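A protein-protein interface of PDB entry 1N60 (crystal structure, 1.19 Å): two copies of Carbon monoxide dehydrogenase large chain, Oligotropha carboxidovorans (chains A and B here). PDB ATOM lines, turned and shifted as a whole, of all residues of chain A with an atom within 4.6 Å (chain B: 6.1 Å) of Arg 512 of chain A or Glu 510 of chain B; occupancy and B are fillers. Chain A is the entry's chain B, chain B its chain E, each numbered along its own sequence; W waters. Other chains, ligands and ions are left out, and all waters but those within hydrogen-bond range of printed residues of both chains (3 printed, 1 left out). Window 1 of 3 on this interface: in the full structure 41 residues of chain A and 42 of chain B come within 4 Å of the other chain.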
ATOM      1  N   GLU A 510       8.960 -32.435   5.824  1.00  0.00           N
ATOM      2  CA  GLU A 510       7.795 -31.857   5.161  1.00  0.00           C
ATOM      3  C   GLU A 510       7.926 -32.238   3.707  1.00  0.00           C
ATOM      4  O   GLU A 510       8.964 -32.067   3.105  1.00  0.00           O
ATOM      5  CB  GLU A 510       7.826 -30.309   5.295  1.00  0.00           C
ATOM      6  CG  GLU A 510       6.647 -29.724   4.582  1.00  0.00           C
ATOM      7  CD  GLU A 510       6.262 -28.348   5.033  1.00  0.00           C
ATOM      8  OE1 GLU A 510       7.105 -27.558   5.432  1.00  0.00           O
ATOM      9  OE2 GLU A 510       5.072 -28.029   4.951  1.00  0.00           O
ATOM     10  N   ILE A 511       6.851 -32.758   3.122  1.00  0.00           N
ATOM     11  CA  ILE A 511       6.853 -33.265   1.765  1.00  0.00           C
ATOM     12  C   ILE A 511       5.678 -32.644   1.063  1.00  0.00           C
ATOM     13  O   ILE A 511       4.561 -32.731   1.522  1.00  0.00           O
ATOM     14  CB  ILE A 511       6.657 -34.791   1.764  1.00  0.00           C
ATOM     15  CG1 ILE A 511       7.733 -35.503   2.593  1.00  0.00           C
ATOM     16  CG2 ILE A 511       6.627 -35.298   0.353  1.00  0.00           C
ATOM     17  CD1 ILE A 511       7.476 -36.969   2.734  1.00  0.00           C
ATOM     18  N   ARG A 512       5.912 -32.027  -0.095  1.00  0.00           N
ATOM     19  CA  ARG A 512       4.889 -31.373  -0.865  1.00  0.00           C
ATOM     20  C   ARG A 512       4.942 -31.901  -2.290  1.00  0.00           C
ATOM     21  O   ARG A 512       5.963 -31.838  -2.952  1.00  0.00           O
ATOM     22  CB  ARG A 512       5.102 -29.830  -0.844  1.00  0.00           C
ATOM     23  CG  ARG A 512       4.130 -29.073  -1.691  1.00  0.00           C
ATOM     24  CD  ARG A 512       4.288 -27.550  -1.518  1.00  0.00           C
ATOM     25  NE  ARG A 512       3.788 -27.181  -0.222  1.00  0.00           N
ATOM     26  CZ  ARG A 512       4.440 -26.489   0.665  1.00  0.00           C
ATOM     27  NH1 ARG A 512       5.571 -25.886   0.399  1.00  0.00           N
ATOM     28  NH2 ARG A 512       3.917 -26.392   1.890  1.00  0.00           N
ATOM     29  N   ILE A 513       3.788 -32.399  -2.768  1.00  0.00           N
ATOM     30  CA  ILE A 513       3.709 -32.912  -4.107  1.00  0.00           C
ATOM     31  C   ILE A 513       3.097 -31.848  -4.991  1.00  0.00           C
ATOM     32  O   ILE A 513       2.059 -31.291  -4.694  1.00  0.00           O
ATOM     33  CB  ILE A 513       2.828 -34.208  -4.187  1.00  0.00           C
ATOM     34  CG1 ILE A 513       2.991 -35.124  -2.956  1.00  0.00           C
ATOM     35  CG2 ILE A 513       3.123 -34.917  -5.515  1.00  0.00           C
ATOM     36  CD1 ILE A 513       4.273 -35.762  -2.882  1.00  0.00           C
ATOM     37  N   HIS A 514       3.747 -31.540  -6.104  1.00  0.00           N
ATOM     38  CA  HIS A 514       3.274 -30.575  -7.035  1.00  0.00           C
ATOM     39  C   HIS A 514       2.207 -31.113  -7.930  1.00  0.00           C
ATOM     40  O   HIS A 514       2.020 -32.321  -8.038  1.00  0.00           O
ATOM     41  CB  HIS A 514       4.454 -30.126  -7.853  1.00  0.00           C
ATOM     42  CG  HIS A 514       5.521 -29.489  -7.044  1.00  0.00           C
ATOM     43  ND1 HIS A 514       5.232 -28.639  -6.008  1.00  0.00           N
ATOM     44  CD2 HIS A 514       6.864 -29.507  -7.168  1.00  0.00           C
ATOM     45  CE1 HIS A 514       6.365 -28.174  -5.494  1.00  0.00           C
ATOM     46  NE2 HIS A 514       7.359 -28.663  -6.208  1.00  0.00           N
ATOM     47  N   SER A 518       5.887 -34.078  -9.259  1.00  0.00           N
ATOM     48  CA  SER A 518       7.180 -33.979  -8.652  1.00  0.00           C
ATOM     49  C   SER A 518       7.023 -33.458  -7.252  1.00  0.00           C
ATOM     50  O   SER A 518       5.928 -33.108  -6.837  1.00  0.00           O
ATOM     51  CB  SER A 518       8.103 -33.170  -9.514  1.00  0.00           C
ATOM     52  OG  SER A 518       7.576 -31.888  -9.745  1.00  0.00           O
ATOM     53  N   VAL A 519       8.125 -33.409  -6.514  1.00  0.00           N
ATOM     54  CA  VAL A 519       8.064 -33.236  -5.060  1.00  0.00           C
ATOM     55  C   VAL A 519       9.185 -32.347  -4.581  1.00  0.00           C
ATOM     56  O   VAL A 519      10.307 -32.503  -5.027  1.00  0.00           O
ATOM     57  CB  VAL A 519       8.209 -34.610  -4.377  1.00  0.00           C
ATOM     58  CG1 VAL A 519       8.146 -34.533  -2.883  1.00  0.00           C
ATOM     59  CG2 VAL A 519       7.219 -35.566  -4.946  1.00  0.00           C
ATOM     60  N   ILE A 520       8.870 -31.521  -3.618  1.00  0.00           N
ATOM     61  CA  ILE A 520       9.872 -30.827  -2.790  1.00  0.00           C
ATOM     62  C   ILE A 520       9.685 -31.331  -1.369  1.00  0.00           C
ATOM     63  O   ILE A 520       8.586 -31.326  -0.835  1.00  0.00           O
ATOM     64  CB  ILE A 520       9.816 -29.301  -2.902  1.00  0.00           C
ATOM     65  CG1 ILE A 520      10.835 -28.671  -1.965  1.00  0.00           C
ATOM     66  CG2 ILE A 520       8.413 -28.776  -2.594  1.00  0.00           C
ATOM     67  CD1 ILE A 520      12.196 -28.884  -2.261  1.00  0.00           C
ATOM     68  N   LEU A 644      -1.590 -31.867  -1.858  1.00  0.00           N
ATOM     69  CA  LEU A 644      -1.130 -33.147  -1.410  1.00  0.00           C
ATOM     70  C   LEU A 644       0.239 -32.978  -0.803  1.00  0.00           C
ATOM     71  O   LEU A 644       1.246 -32.924  -1.507  1.00  0.00           O
ATOM     72  CB  LEU A 644      -1.126 -34.103  -2.589  1.00  0.00           C
ATOM     73  CG  LEU A 644      -0.887 -35.541  -2.220  1.00  0.00           C
ATOM     74  CD1 LEU A 644      -1.915 -36.116  -1.311  1.00  0.00           C
ATOM     75  CD2 LEU A 644      -0.892 -36.378  -3.492  1.00  0.00           C
ATOM     76  N   GLU A 645       0.242 -32.854   0.528  1.00  0.00           N
ATOM     77  CA  GLU A 645       1.456 -32.591   1.234  1.00  0.00           C
ATOM     78  C   GLU A 645       1.308 -33.039   2.671  1.00  0.00           C
ATOM     79  O   GLU A 645       0.205 -33.220   3.133  1.00  0.00           O
ATOM     80  CB  GLU A 645       1.809 -31.129   1.134  1.00  0.00           C
ATOM     81  CG  GLU A 645       0.775 -30.173   1.702  1.00  0.00           C
ATOM     82  CD  GLU A 645       1.269 -28.786   1.460  1.00  0.00           C
ATOM     83  OE1 GLU A 645       1.275 -28.311   0.286  1.00  0.00           O
ATOM     84  OE2 GLU A 645       1.711 -28.149   2.410  1.00  0.00           O
ATOM     85  N   VAL A 647       3.505 -33.014   6.795  1.00  0.00           N
ATOM     86  CA  VAL A 647       4.606 -32.831   7.677  1.00  0.00           C
ATOM     87  C   VAL A 647       4.527 -33.871   8.776  1.00  0.00           C
ATOM     88  O   VAL A 647       3.433 -34.268   9.187  1.00  0.00           O
ATOM     89  CB  VAL A 647       4.496 -31.421   8.351  1.00  0.00           C
ATOM     90  CG1 VAL A 647       5.507 -31.212   9.434  1.00  0.00           C
ATOM     91  CG2 VAL A 647       4.576 -30.365   7.357  1.00  0.00           C
ATOM     92  N   SER B 508      -3.962 -20.719  -0.154  1.00  0.00           N
ATOM     93  CA  SER B 508      -3.284 -21.479   0.883  1.00  0.00           C
ATOM     94  C   SER B 508      -2.479 -20.616   1.815  1.00  0.00           C
ATOM     95  O   SER B 508      -2.035 -19.531   1.454  1.00  0.00           O
ATOM     96  CB  SER B 508      -2.376 -22.504   0.218  1.00  0.00           C
ATOM     97  OG  SER B 508      -1.415 -21.845  -0.530  1.00  0.00           O
ATOM     98  N   ALA B 509      -2.226 -21.210   2.985  1.00  0.00           N
ATOM     99  CA  ALA B 509      -1.395 -20.612   3.990  1.00  0.00           C
ATOM    100  C   ALA B 509      -0.686 -21.703   4.727  1.00  0.00           C
ATOM    101  O   ALA B 509      -1.301 -22.722   5.067  1.00  0.00           O
ATOM    102  CB  ALA B 509      -2.180 -19.720   4.977  1.00  0.00           C
ATOM    103  N   GLU B 510       0.545 -21.461   5.109  1.00  0.00           N
ATOM    104  CA  GLU B 510       1.306 -22.320   6.003  1.00  0.00           C
ATOM    105  C   GLU B 510       1.880 -21.418   7.055  1.00  0.00           C
ATOM    106  O   GLU B 510       2.493 -20.421   6.753  1.00  0.00           O
ATOM    107  CB  GLU B 510       2.406 -23.010   5.217  1.00  0.00           C
ATOM    108  CG  GLU B 510       3.285 -23.885   6.148  1.00  0.00           C
ATOM    109  CD  GLU B 510       4.060 -24.955   5.442  1.00  0.00           C
ATOM    110  OE1 GLU B 510       4.476 -24.773   4.298  1.00  0.00           O
ATOM    111  OE2 GLU B 510       4.220 -26.033   6.063  1.00  0.00           O
ATOM    112  N   ILE B 511       1.698 -21.831   8.296  1.00  0.00           N
ATOM    113  CA  ILE B 511       2.135 -21.032   9.438  1.00  0.00           C
ATOM    114  C   ILE B 511       2.979 -21.922  10.310  1.00  0.00           C
ATOM    115  O   ILE B 511       2.501 -22.972  10.737  1.00  0.00           O
ATOM    116  CB  ILE B 511       0.926 -20.517  10.212  1.00  0.00           C
ATOM    117  CG1 ILE B 511      -0.045 -19.725   9.315  1.00  0.00           C
ATOM    118  CG2 ILE B 511       1.387 -19.718  11.408  1.00  0.00           C
ATOM    119  CD1 ILE B 511      -1.283 -19.305  10.038  1.00  0.00           C
ATOM    120  N   ARG B 512       4.153 -21.482  10.713  1.00  0.00           N
ATOM    121  CA  ARG B 512       5.044 -22.253  11.572  1.00  0.00           C
ATOM    122  C   ARG B 512       5.504 -21.349  12.679  1.00  0.00           C
ATOM    123  O   ARG B 512       6.033 -20.282  12.459  1.00  0.00           O
ATOM    124  CB  ARG B 512       6.228 -22.765  10.740  1.00  0.00           C
ATOM    125  CG  ARG B 512       7.305 -23.449  11.539  1.00  0.00           C
ATOM    126  CD  ARG B 512       8.400 -24.028  10.693  1.00  0.00           C
ATOM    127  NE  ARG B 512       7.866 -25.145   9.932  1.00  0.00           N
ATOM    128  CZ  ARG B 512       7.918 -25.291   8.638  1.00  0.00           C
ATOM    129  NH1 ARG B 512       8.697 -24.530   7.876  1.00  0.00           N
ATOM    130  NH2 ARG B 512       7.268 -26.309   8.097  1.00  0.00           N
ATOM    131  N   ILE B 520       6.897 -17.848  11.023  1.00  0.00           N
ATOM    132  CA  ILE B 520       7.030 -17.666   9.589  1.00  0.00           C
ATOM    133  C   ILE B 520       5.780 -18.194   8.967  1.00  0.00           C
ATOM    134  O   ILE B 520       5.379 -19.309   9.268  1.00  0.00           O
ATOM    135  CB  ILE B 520       8.297 -18.350   9.008  1.00  0.00           C
ATOM    136  CG1 ILE B 520       8.374 -18.218   7.490  1.00  0.00           C
ATOM    137  CG2 ILE B 520       8.439 -19.814   9.413  1.00  0.00           C
ATOM    138  CD1 ILE B 520       8.485 -16.851   7.002  1.00  0.00           C
ATOM    139  N   ALA B 521       5.166 -17.405   8.115  1.00  0.00           N
ATOM    140  CA  ALA B 521       3.957 -17.812   7.437  1.00  0.00           C
ATOM    141  C   ALA B 521       4.067 -17.410   5.981  1.00  0.00           C
ATOM    142  O   ALA B 521       4.639 -16.387   5.618  1.00  0.00           O
ATOM    143  CB  ALA B 521       2.779 -17.161   8.049  1.00  0.00           C
ATOM    144  N   ARG B 522       3.597 -18.303   5.121  1.00  0.00           N
ATOM    145  CA  ARG B 522       3.616 -18.073   3.698  1.00  0.00           C
ATOM    146  C   ARG B 522       2.283 -18.389   3.098  1.00  0.00           C
ATOM    147  O   ARG B 522       1.559 -19.221   3.637  1.00  0.00           O
ATOM    148  CB  ARG B 522       4.674 -18.956   3.042  1.00  0.00           C
ATOM    149  CG  ARG B 522       6.040 -18.756   3.567  1.00  0.00           C
ATOM    150  CD  ARG B 522       7.076 -19.332   2.676  1.00  0.00           C
ATOM    151  NE  ARG B 522       8.403 -19.012   3.156  1.00  0.00           N
ATOM    152  CZ  ARG B 522       9.071 -19.682   4.042  1.00  0.00           C
ATOM    153  NH1 ARG B 522       8.602 -20.848   4.465  1.00  0.00           N
ATOM    154  NH2 ARG B 522      10.301 -19.231   4.380  1.00  0.00           N
ATOM    155  N   MET B 523       1.970 -17.753   1.981  1.00  0.00           N
ATOM    156  CA  MET B 523       0.704 -17.852   1.364  1.00  0.00           C
ATOM    157  C   MET B 523       0.896 -18.042  -0.130  1.00  0.00           C
ATOM    158  O   MET B 523       1.955 -17.675  -0.661  1.00  0.00           O
ATOM    159  CB  MET B 523      -0.185 -16.664   1.656  1.00  0.00           C
ATOM    160  CG  MET B 523      -0.635 -16.530   3.086  1.00  0.00           C
ATOM    161  SD  MET B 523       0.658 -15.916   4.192  1.00  0.00           S
ATOM    162  CE  MET B 523      -0.144 -16.196   5.750  1.00  0.00           C
ATOM    163  N   THR B 558       8.083 -20.109  -5.362  1.00  0.00           N
ATOM    164  CA  THR B 558       7.298 -21.307  -5.509  1.00  0.00           C
ATOM    165  C   THR B 558       7.933 -22.487  -4.852  1.00  0.00           C
ATOM    166  O   THR B 558       7.263 -23.495  -4.602  1.00  0.00           O
ATOM    167  CB  THR B 558       7.019 -21.628  -6.981  1.00  0.00           C
ATOM    168  OG1 THR B 558       8.228 -21.822  -7.710  1.00  0.00           O
ATOM    169  CG2 THR B 558       6.225 -20.465  -7.601  1.00  0.00           C
ATOM    170  N   ASP B 559       9.219 -22.424  -4.551  1.00  0.00           N
ATOM    171  CA  ASP B 559       9.823 -23.484  -3.795  1.00  0.00           C
ATOM    172  C   ASP B 559       9.349 -23.498  -2.359  1.00  0.00           C
ATOM    173  O   ASP B 559       9.349 -24.557  -1.710  1.00  0.00           O
ATOM    174  CB  ASP B 559      11.328 -23.323  -3.739  1.00  0.00           C
ATOM    175  CG  ASP B 559      12.072 -23.627  -4.959  1.00  0.00           C
ATOM    176  OD1 ASP B 559      11.563 -24.137  -5.963  1.00  0.00           O
ATOM    177  OD2 ASP B 559      13.314 -23.397  -4.933  1.00  0.00           O
ATOM    178  N   THR B 560       8.980 -22.342  -1.813  1.00  0.00           N
ATOM    179  CA  THR B 560       8.760 -22.219  -0.376  1.00  0.00           C
ATOM    180  C   THR B 560       7.307 -21.992   0.002  1.00  0.00           C
ATOM    181  O   THR B 560       6.816 -22.524   0.977  1.00  0.00           O
ATOM    182  CB  THR B 560       9.613 -21.172   0.227  1.00  0.00           C
ATOM    183  OG1 THR B 560       9.223 -19.862  -0.224  1.00  0.00           O
ATOM    184  CG2 THR B 560      11.087 -21.401  -0.139  1.00  0.00           C
ATOM    185  N   ALA B 561       6.610 -21.153  -0.725  1.00  0.00           N
ATOM    186  CA  ALA B 561       5.245 -20.870  -0.425  1.00  0.00           C
ATOM    187  C   ALA B 561       4.347 -21.988  -0.830  1.00  0.00           C
ATOM    188  O   ALA B 561       4.597 -22.687  -1.811  1.00  0.00           O
ATOM    189  CB  ALA B 561       4.833 -19.610  -1.167  1.00  0.00           C
ATOM    190  N   PRO B 562       3.315 -22.262  -0.053  1.00  0.00           N
ATOM    191  CA  PRO B 562       2.399 -23.318  -0.435  1.00  0.00           C
ATOM    192  C   PRO B 562       1.760 -22.952  -1.765  1.00  0.00           C
ATOM    193  O   PRO B 562       1.718 -21.779  -2.165  1.00  0.00           O
ATOM    194  CB  PRO B 562       1.379 -23.307   0.703  1.00  0.00           C
ATOM    195  CG  PRO B 562       1.374 -21.866   1.206  1.00  0.00           C
ATOM    196  CD  PRO B 562       2.824 -21.459   1.070  1.00  0.00           C
ATOM    197  N   TYR B 563       1.322 -23.940  -2.528  1.00  0.00           N
ATOM    198  CA  TYR B 563       0.769 -23.658  -3.834  1.00  0.00           C
ATOM    199  C   TYR B 563      -0.432 -22.790  -3.693  1.00  0.00           C
ATOM    200  O   TYR B 563      -1.309 -23.106  -2.905  1.00  0.00           O
ATOM    201  CB  TYR B 563       0.391 -24.967  -4.570  1.00  0.00           C
ATOM    202  CG  TYR B 563       0.248 -24.826  -6.057  1.00  0.00           C
ATOM    203  CD1 TYR B 563      -0.908 -24.292  -6.614  1.00  0.00           C
ATOM    204  CD2 TYR B 563       1.255 -25.216  -6.916  1.00  0.00           C
ATOM    205  CE1 TYR B 563      -1.005 -24.126  -7.991  1.00  0.00           C
ATOM    206  CE2 TYR B 563       1.151 -25.065  -8.251  1.00  0.00           C
ATOM    207  CZ  TYR B 563       0.022 -24.551  -8.805  1.00  0.00           C
ATOM    208  OH  TYR B 563      -0.109 -24.382 -10.170  1.00  0.00           O
ATOM    209  N   ALA B 583      -5.663 -22.067   9.014  1.00  0.00           N
ATOM    210  CA  ALA B 583      -4.415 -22.591   9.469  1.00  0.00           C
ATOM    211  C   ALA B 583      -4.112 -22.142  10.883  1.00  0.00           C
ATOM    212  O   ALA B 583      -3.663 -22.955  11.706  1.00  0.00           O
ATOM    213  CB  ALA B 583      -3.306 -22.222   8.506  1.00  0.00           C
ATOM    214  N   GLU B 645       2.630 -25.892  14.064  1.00  0.00           N
ATOM    215  CA  GLU B 645       2.535 -25.373  12.721  1.00  0.00           C
ATOM    216  C   GLU B 645       1.299 -25.956  12.036  1.00  0.00           C
ATOM    217  O   GLU B 645       0.794 -26.968  12.484  1.00  0.00           O
ATOM    218  CB  GLU B 645       3.745 -25.677  11.888  1.00  0.00           C
ATOM    219  CG  GLU B 645       4.091 -27.154  11.755  1.00  0.00           C
ATOM    220  CD  GLU B 645       5.377 -27.257  10.999  1.00  0.00           C
ATOM    221  OE1 GLU B 645       6.438 -26.930  11.588  1.00  0.00           O
ATOM    222  OE2 GLU B 645       5.352 -27.572   9.793  1.00  0.00           O
ATOM    223  N   ALA B 646       0.866 -25.347  10.953  1.00  0.00           N
ATOM    224  CA  ALA B 646      -0.230 -25.890  10.207  1.00  0.00           C
ATOM    225  C   ALA B 646      -0.286 -25.280   8.835  1.00  0.00           C
ATOM    226  O   ALA B 646       0.285 -24.205   8.544  1.00  0.00           O
ATOM    227  CB  ALA B 646      -1.558 -25.549  10.889  1.00  0.00           C
ATOM    228  N   VAL B 647      -0.944 -25.991   7.971  1.00  0.00           N
ATOM    229  CA  VAL B 647      -1.203 -25.571   6.585  1.00  0.00           C
ATOM    230  C   VAL B 647      -2.693 -25.658   6.362  1.00  0.00           C
ATOM    231  O   VAL B 647      -3.369 -26.556   6.919  1.00  0.00           O
ATOM    232  CB  VAL B 647      -0.512 -26.571   5.637  1.00  0.00           C
ATOM    233  CG1 VAL B 647      -0.985 -26.386   4.263  1.00  0.00           C
ATOM    234  CG2 VAL B 647       0.957 -26.501   5.776  1.00  0.00           C
ATOM    235  N   ASN B 648      -3.253 -24.792   5.534  1.00  0.00           N
ATOM    236  CA  ASN B 648      -4.568 -24.931   5.047  1.00  0.00           C
ATOM    237  C   ASN B 648      -4.578 -24.537   3.589  1.00  0.00           C
ATOM    238  O   ASN B 648      -4.029 -23.505   3.202  1.00  0.00           O
ATOM    239  CB  ASN B 648      -5.571 -24.093   5.810  1.00  0.00           C
ATOM    240  CG  ASN B 648      -6.989 -24.197   5.257  1.00  0.00           C
ATOM    241  OD1 ASN B 648      -7.507 -23.237   4.713  1.00  0.00           O
ATOM    242  ND2 ASN B 648      -7.578 -25.365   5.357  1.00  0.00           N
ATOM    243  N   TYR B 649      -5.205 -25.400   2.787  1.00  0.00           N
ATOM    244  CA  TYR B 649      -5.572 -25.051   1.402  1.00  0.00           C
ATOM    245  C   TYR B 649      -7.066 -24.899   1.414  1.00  0.00           C
ATOM    246  O   TYR B 649      -7.782 -25.844   1.704  1.00  0.00           O
ATOM    247  CB  TYR B 649      -5.167 -26.148   0.433  1.00  0.00           C
ATOM    248  CG  TYR B 649      -3.703 -26.222   0.108  1.00  0.00           C
ATOM    249  CD1 TYR B 649      -2.705 -26.194   1.037  1.00  0.00           C
ATOM    250  CD2 TYR B 649      -3.290 -26.263  -1.217  1.00  0.00           C
ATOM    251  CE1 TYR B 649      -1.352 -26.244   0.674  1.00  0.00           C
ATOM    252  CE2 TYR B 649      -1.990 -26.290  -1.575  1.00  0.00           C
ATOM    253  CZ  TYR B 649      -1.005 -26.284  -0.649  1.00  0.00           C
ATOM    254  OH  TYR B 649       0.280 -26.319  -1.030  1.00  0.00           O
HETATM  255  O   HOH W   1       0.016 -29.532  -1.889  1.00  0.00           O
HETATM  256  O   HOH W   2       7.384 -25.013   2.532  1.00  0.00           O
HETATM  257  O   HOH W   3       8.339 -24.345   4.943  1.00  0.00           O
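Of the printed residues of chain B, Arg 512 of chain A touches Glu 510, Thr 560, Pro 562 and Tyr 649. Ser 518 of chain A touches none of the printed residues of chain B. Glu 510 of chain B touches just these residues of chain A: Glu 510 (2.4 Å) and Arg 512 (3.0 Å). Of the printed residues of chain A, Arg 512 of chain B touches Glu 510 (2.9 Å). Printed residues of chain A within 4 Å of Thr 560 of chain B: Arg 512 (3.6 Å). Tyr 563 of chain B touches none of the printed residues of chain A. Printed residues of chain A within 4 Å of Glu 645 of chain B: Val 647. Printed residues of chain A within 4 Å of Val 647 of chain B: Glu 645. The nearest printed residue of chain B that does not touch Val 647 of chain A is Glu 510 of chain B (4.5 Å).
The guanidinium group (NH2) of Arg 512 of chain B is in salt-bridge range of the side-chain carboxylate (OE2) of Glu 510 of chain B, at 3.7 Å. The backbone NH (N) of Tyr 563 of chain B is in hydrogen-bond range of the side-chain hydroxyl (OH) of Tyr 649 of chain B, at 3.0 Å. NH2 of Arg 512 of chain A is in salt-bridge range of OE2 of Glu 510 of chain A, at 3.7 Å. The guanidinium group of Arg 512 of chain B is in salt-bridge range of the side-chain carboxylate of Glu 645 of chain B (2.8 Å). The backbone NH (N) of Glu 510 of chain B lies within hydrogen-bond range of the backbone carbonyl oxygen (O) of Arg 522 of chain B (2.9 Å). The guanidinium group of Arg 512 of chain A lies within salt-bridge range of the side-chain carboxylate of Glu 645 of chain A (2.8 Å).
Water W1 lies within hydrogen-bond range of the side-chain carboxylate of Glu 645 of chain A, the backbone NH of Leu 644 of chain A and the side-chain hydroxyl of Tyr 649 of chain B. Water W2 lies within hydrogen-bond range of NH1 of Arg 512 of chain A (2.9 Å), O of Thr 560 of chain B (3.0 Å) and OE1 of Glu 510 of chain B (3.4 Å). Water W3 bridges the guanidinium group (NH1) of Arg 512 of chain B and the side-chain carboxylate (OE1) of Glu 510 of chain A.
Arg 512 of chain A touches Thr 560 of chain B (NH1 to O, 3.6 Å). Pro 562 of chain B touches Arg 512 of chain A (CA to CZ, 3.9 Å). Arg 512 of chain A touches Tyr 649 of chain B. Glu 645 of chain A touches Val 647 of chain B (OE2 to CG1, 3.7 Å). OE2 of Glu 645 of chain B touches CG1 of Val 647 of chain A (3.7 Å).
Hydrophobic or aromatic side chains of chain B that line the printed part of chain A: Val 647 and Tyr 649. Of the 11 printed residues of chain A, 4 touch a printed residue of chain B. Hydrophobic or aromatic side chains of chain A that line the printed part of chain B: Val 647. Among the printed residues, 9 pairs touch across the chains.
Glu 510 of chain B touches its own counterpart, Glu 510 of chain A. Glu 510 of chain A touches Arg 512 of chain B, and with the chains exchanged Arg 512 of chain A touches Glu 510 of chain B. Glu 645 of chain A touches Val 647 of chain B, and with the chains exchanged Val 647 of chain A touches Glu 645 of chain B. Positions printed for both chains: 510, 511, 512, 520, 645 and 647.
OE1 of Glu 645 of chain A sits at hydrogen-bond distance from OH of Tyr 649 of chain B (2.6 Å). OE2 of Glu 510 of chain A lies close to OE2 of Glu 510 of chain B (2.4 Å). The side-chain carboxylate (OE1) of Glu 510 of chain A is in salt-bridge range of the guanidinium group (NH2) of Arg 512 of chain B, 2.9 Å away. OE1 of Glu 510 of chain B lies within salt-bridge range of NH2 of Arg 512 of chain A (3.0 Å).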
